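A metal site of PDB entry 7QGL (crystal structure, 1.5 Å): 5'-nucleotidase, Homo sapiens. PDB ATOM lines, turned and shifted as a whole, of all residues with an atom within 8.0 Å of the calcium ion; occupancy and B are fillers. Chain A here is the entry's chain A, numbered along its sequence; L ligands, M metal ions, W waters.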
ATOM      1  N   LYS A 182      20.924  25.481  28.555  1.00  0.00           N
ATOM      2  CA  LYS A 182      19.600  25.030  28.134  1.00  0.00           C
ATOM      3  C   LYS A 182      18.522  26.065  28.463  1.00  0.00           C
ATOM      4  O   LYS A 182      17.582  26.209  27.701  1.00  0.00           O
ATOM      5  CB  LYS A 182      19.266  23.685  28.778  1.00  0.00           C
ATOM      6  CG  LYS A 182      20.056  22.533  28.191  1.00  0.00           C
ATOM      7  CD  LYS A 182      19.650  22.237  26.754  1.00  0.00           C
ATOM      8  CE  LYS A 182      19.892  20.795  26.369  1.00  0.00           C
ATOM      9  NZ  LYS A 182      19.460  20.489  24.957  1.00  0.00           N
ATOM     10  N   VAL A 186      19.846  27.381  24.226  1.00  0.00           N
ATOM     11  CA  VAL A 186      20.949  26.852  23.429  1.00  0.00           C
ATOM     12  C   VAL A 186      20.722  25.356  23.415  1.00  0.00           C
ATOM     13  O   VAL A 186      20.728  24.739  24.472  1.00  0.00           O
ATOM     14  CB  VAL A 186      22.309  27.213  24.040  1.00  0.00           C
ATOM     15  CG1 VAL A 186      23.444  26.559  23.232  1.00  0.00           C
ATOM     16  CG2 VAL A 186      22.468  28.725  24.113  1.00  0.00           C
ATOM     17  N   ASN A 187      20.425  24.789  22.230  1.00  0.00           N
ATOM     18  CA  ASN A 187      20.077  23.370  22.139  1.00  0.00           C
ATOM     19  C   ASN A 187      21.147  22.480  21.541  1.00  0.00           C
ATOM     20  O   ASN A 187      20.932  21.285  21.423  1.00  0.00           O
ATOM     21  CB  ASN A 187      18.740  23.205  21.390  1.00  0.00           C
ATOM     22  CG  ASN A 187      18.744  23.726  19.975  1.00  0.00           C
ATOM     23  OD1 ASN A 187      19.689  23.519  19.214  1.00  0.00           O
ATOM     24  ND2 ASN A 187      17.651  24.367  19.549  1.00  0.00           N
ATOM     25  N   LYS A 188      22.288  23.051  21.146  1.00  0.00           N
ATOM     26  CA  LYS A 188      23.407  22.290  20.578  1.00  0.00           C
ATOM     27  C   LYS A 188      24.612  22.616  21.446  1.00  0.00           C
ATOM     28  O   LYS A 188      24.983  23.778  21.588  1.00  0.00           O
ATOM     29  CB  LYS A 188      23.634  22.697  19.124  1.00  0.00           C
ATOM     30  CG  LYS A 188      22.488  22.213  18.230  1.00  0.00           C
ATOM     31  CD  LYS A 188      22.665  22.690  16.794  1.00  0.00           C
ATOM     32  CE  LYS A 188      22.261  24.140  16.631  1.00  0.00           C
ATOM     33  NZ  LYS A 188      20.780  24.309  16.788  1.00  0.00           N
ATOM     34  N   ILE A 189      25.124  21.599  22.160  1.00  0.00           N
ATOM     35  CA  ILE A 189      26.160  21.822  23.153  1.00  0.00           C
ATOM     36  C   ILE A 189      27.288  20.844  22.994  1.00  0.00           C
ATOM     37  O   ILE A 189      27.069  19.645  22.965  1.00  0.00           O
ATOM     38  CB  ILE A 189      25.545  21.713  24.560  1.00  0.00           C
ATOM     39  CG1 ILE A 189      24.478  22.821  24.776  1.00  0.00           C
ATOM     40  CG2 ILE A 189      26.642  21.837  25.634  1.00  0.00           C
ATOM     41  CD1 ILE A 189      23.652  22.684  26.043  1.00  0.00           C
ATOM     42  N   ILE A 190      28.514  21.397  22.912  1.00  0.00           N
ATOM     43  CA  ILE A 190      29.732  20.614  22.828  1.00  0.00           C
ATOM     44  C   ILE A 190      30.462  20.728  24.148  1.00  0.00           C
ATOM     45  O   ILE A 190      30.656  21.845  24.629  1.00  0.00           O
ATOM     46  CB  ILE A 190      30.639  21.206  21.711  1.00  0.00           C
ATOM     47  CG1 ILE A 190      29.938  21.181  20.347  1.00  0.00           C
ATOM     48  CG2 ILE A 190      31.976  20.478  21.681  1.00  0.00           C
ATOM     49  CD1 ILE A 190      30.685  21.875  19.254  1.00  0.00           C
ATOM     50  N   GLY A 209      22.447  16.775  28.492  1.00  0.00           N
ATOM     51  CA  GLY A 209      22.434  17.915  27.589  1.00  0.00           C
ATOM     52  C   GLY A 209      23.647  18.048  26.704  1.00  0.00           C
ATOM     53  O   GLY A 209      23.628  18.880  25.786  1.00  0.00           O
ATOM     54  N   VAL A 210      24.709  17.290  26.960  1.00  0.00           N
ATOM     55  CA  VAL A 210      25.906  17.336  26.112  1.00  0.00           C
ATOM     56  C   VAL A 210      25.660  16.516  24.845  1.00  0.00           C
ATOM     57  O   VAL A 210      25.313  15.337  24.926  1.00  0.00           O
ATOM     58  CB  VAL A 210      27.135  16.803  26.906  1.00  0.00           C
ATOM     59  CG1 VAL A 210      28.320  16.519  25.981  1.00  0.00           C
ATOM     60  CG2 VAL A 210      27.526  17.803  27.975  1.00  0.00           C
ATOM     61  N   ASP A 211      25.838  17.154  23.667  1.00  0.00           N
ATOM     62  CA  ASP A 211      25.599  16.437  22.410  1.00  0.00           C
ATOM     63  C   ASP A 211      26.825  15.737  21.858  1.00  0.00           C
ATOM     64  O   ASP A 211      26.686  14.746  21.136  1.00  0.00           O
ATOM     65  CB  ASP A 211      25.069  17.424  21.357  1.00  0.00           C
ATOM     66  CG  ASP A 211      23.734  18.012  21.741  1.00  0.00           C
ATOM     67  OD1 ASP A 211      22.790  17.241  21.953  1.00  0.00           O
ATOM     68  OD2 ASP A 211      23.614  19.252  21.762  1.00  0.00           O
ATOM     69  N   VAL A 212      28.015  16.215  22.220  1.00  0.00           N
ATOM     70  CA  VAL A 212      29.268  15.640  21.735  1.00  0.00           C
ATOM     71  C   VAL A 212      30.367  16.046  22.686  1.00  0.00           C
ATOM     72  O   VAL A 212      30.302  17.104  23.323  1.00  0.00           O
ATOM     73  CB  VAL A 212      29.574  16.131  20.290  1.00  0.00           C
ATOM     74  CG1 VAL A 212      29.536  17.649  20.219  1.00  0.00           C
ATOM     75  CG2 VAL A 212      30.894  15.580  19.737  1.00  0.00           C
ATOM     76  N   ARG A 247      20.466   8.886  24.939  1.00  0.00           N
ATOM     77  CA  ARG A 247      20.978   9.468  23.694  1.00  0.00           C
ATOM     78  C   ARG A 247      22.306   8.818  23.323  1.00  0.00           C
ATOM     79  O   ARG A 247      22.995   8.282  24.172  1.00  0.00           O
ATOM     80  CB  ARG A 247      21.177  10.983  23.847  1.00  0.00           C
ATOM     81  CG  ARG A 247      19.870  11.733  24.115  1.00  0.00           C
ATOM     82  CD  ARG A 247      20.163  13.183  24.496  1.00  0.00           C
ATOM     83  NE  ARG A 247      20.753  13.272  25.834  1.00  0.00           N
ATOM     84  CZ  ARG A 247      22.014  13.633  26.088  1.00  0.00           C
ATOM     85  NH1 ARG A 247      22.479  13.629  27.325  1.00  0.00           N
ATOM     86  NH2 ARG A 247      22.834  13.976  25.088  1.00  0.00           N
ATOM     87  N   PHE A 268      22.094  17.554  13.148  1.00  0.00           N
ATOM     88  CA  PHE A 268      21.134  17.908  14.197  1.00  0.00           C
ATOM     89  C   PHE A 268      19.777  18.191  13.581  1.00  0.00           C
ATOM     90  O   PHE A 268      19.688  18.691  12.455  1.00  0.00           O
ATOM     91  CB  PHE A 268      21.540  19.210  14.900  1.00  0.00           C
ATOM     92  CG  PHE A 268      22.785  19.160  15.745  1.00  0.00           C
ATOM     93  CD1 PHE A 268      22.729  18.758  17.066  1.00  0.00           C
ATOM     94  CD2 PHE A 268      24.001  19.579  15.230  1.00  0.00           C
ATOM     95  CE1 PHE A 268      23.864  18.763  17.854  1.00  0.00           C
ATOM     96  CE2 PHE A 268      25.144  19.563  16.016  1.00  0.00           C
ATOM     97  CZ  PHE A 268      25.059  19.185  17.331  1.00  0.00           C
ATOM     98  N   ASP A 269      18.717  17.917  14.329  1.00  0.00           N
ATOM     99  CA  ASP A 269      17.399  18.353  13.889  1.00  0.00           C
ATOM    100  C   ASP A 269      17.231  19.796  14.424  1.00  0.00           C
ATOM    101  O   ASP A 269      18.136  20.341  15.078  1.00  0.00           O
ATOM    102  CB  ASP A 269      16.287  17.373  14.296  1.00  0.00           C
ATOM    103  CG  ASP A 269      15.950  17.317  15.775  1.00  0.00           C
ATOM    104  OD1 ASP A 269      16.474  18.159  16.539  1.00  0.00           O
ATOM    105  OD2 ASP A 269      15.180  16.415  16.163  1.00  0.00           O
ATOM    106  N   ARG A 271      15.572  20.979  16.813  1.00  0.00           N
ATOM    107  CA  ARG A 271      15.545  21.111  18.266  1.00  0.00           C
ATOM    108  C   ARG A 271      16.888  20.731  18.922  1.00  0.00           C
ATOM    109  O   ARG A 271      16.955  20.589  20.138  1.00  0.00           O
ATOM    110  CB  ARG A 271      14.425  20.262  18.847  1.00  0.00           C
ATOM    111  CG  ARG A 271      13.045  20.526  18.217  1.00  0.00           C
ATOM    112  CD  ARG A 271      11.895  19.837  18.944  1.00  0.00           C
ATOM    113  NE  ARG A 271      12.227  18.485  19.418  1.00  0.00           N
ATOM    114  CZ  ARG A 271      12.508  18.180  20.680  1.00  0.00           C
ATOM    115  NH1 ARG A 271      12.509  19.125  21.613  1.00  0.00           N
ATOM    116  NH2 ARG A 271      12.805  16.935  21.014  1.00  0.00           N
ATOM    117  N   GLY A 272      17.940  20.534  18.123  1.00  0.00           N
ATOM    118  CA  GLY A 272      19.244  20.190  18.656  1.00  0.00           C
ATOM    119  C   GLY A 272      19.448  18.730  19.019  1.00  0.00           C
ATOM    120  O   GLY A 272      20.408  18.410  19.721  1.00  0.00           O
ATOM    121  N   ASN A 273      18.522  17.851  18.604  1.00  0.00           N
ATOM    122  CA  ASN A 273      18.707  16.408  18.835  1.00  0.00           C
ATOM    123  C   ASN A 273      19.728  15.938  17.816  1.00  0.00           C
ATOM    124  O   ASN A 273      19.664  16.349  16.666  1.00  0.00           O
ATOM    125  CB  ASN A 273      17.409  15.660  18.607  1.00  0.00           C
ATOM    126  CG  ASN A 273      16.309  16.051  19.571  1.00  0.00           C
ATOM    127  OD1 ASN A 273      16.497  15.979  20.784  1.00  0.00           O
ATOM    128  ND2 ASN A 273      15.169  16.448  19.055  1.00  0.00           N
ATOM    129  N   VAL A 274      20.632  15.037  18.201  1.00  0.00           N
ATOM    130  CA  VAL A 274      21.632  14.508  17.276  1.00  0.00           C
ATOM    131  C   VAL A 274      21.005  13.341  16.509  1.00  0.00           C
ATOM    132  O   VAL A 274      20.573  12.363  17.124  1.00  0.00           O
ATOM    133  CB  VAL A 274      22.919  14.064  18.004  1.00  0.00           C
ATOM    134  CG1 VAL A 274      23.860  13.323  17.065  1.00  0.00           C
ATOM    135  CG2 VAL A 274      23.618  15.276  18.633  1.00  0.00           C
HETATM  136  O1  LIG L   1      19.872  17.630  25.538  1.00  0.00           O
HETATM  137  C1  LIG L   1      20.494  17.012  24.402  1.00  0.00           C
HETATM  138  C2  LIG L   1      19.587  17.095  23.206  1.00  0.00           C
HETATM  139  O2  LIG L   1      19.340  18.458  22.906  1.00  0.00           O
HETATM  140  C3  LIG L   1      16.904  18.461  22.999  1.00  0.00           C
HETATM  141  C4  LIG L   1      18.149  18.708  22.175  1.00  0.00           C
HETATM  142  O3  LIG L   1      16.927  19.212  24.208  1.00  0.00           O
HETATM  143  C5  LIG L   1      15.775  19.887  26.226  1.00  0.00           C
HETATM  144  C6  LIG L   1      15.738  19.045  24.979  1.00  0.00           C
HETATM  145  O4  LIG L   1      16.768  19.413  27.122  1.00  0.00           O
HETATM  146  C7  LIG L   1      17.346  19.786  29.453  1.00  0.00           C
HETATM  147  C8  LIG L   1      16.313  19.308  28.469  1.00  0.00           C
HETATM  148  O5  LIG L   1      18.653  19.362  29.094  1.00  0.00           O
HETATM  149  C9  LIG L   1      20.383  19.866  30.704  1.00  0.00           C
HETATM  150  C10 LIG L   1      19.430  18.845  30.171  1.00  0.00           C
HETATM  151  O6  LIG L   1      19.761  20.580  31.772  1.00  0.00           O
HETATM  152 CA    CA M   1      21.203  19.010  21.783  1.00  0.00          CA
HETATM  153  O   HOH W   1      22.081  20.106  24.017  1.00  0.00           O
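The backbone NH of Asp 211 is in hydrogen-bond range of the backbone carbonyl oxygen of Ile 189 (2.9 Å). OD1 of Asn 187 sits at hydrogen-bond distance from NZ of Lys 188, at 2.8 Å. The backbone NH (N) of Gly 272 is in hydrogen-bond range of the side-chain carboxylate (OD1) of Asp 269, at 3.2 Å.
Lys 182 touches the calcium ion (NZ to CA, 3.9 Å). Of the 17 residues printed, 4 come within 4 Å of the calcium ion. The nearest printed residue that does not touch the calcium ion is Lys 188 (4.1 Å).
The calcium ion is bound by O2 of the ligand, at 2.2 Å. O of Gly 272 binds the calcium ion (2.3 Å). The calcium ion is bound by the backbone carbonyl oxygen (O) of Asn 187. OD1 of Asp 211 is bound to the calcium ion (2.4 Å). OD2 of Asp 211 binds the calcium ion (2.4 Å). The calcium ion is bound by water W1. The calcium ion has six donor atoms within binding distance.
Water W1 lies within hydrogen-bond range of the backbone carbonyl oxygen (O) of Gly 209 (2.7 Å) and the side-chain amino group (NZ) of Lys 182 (2.8 Å).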
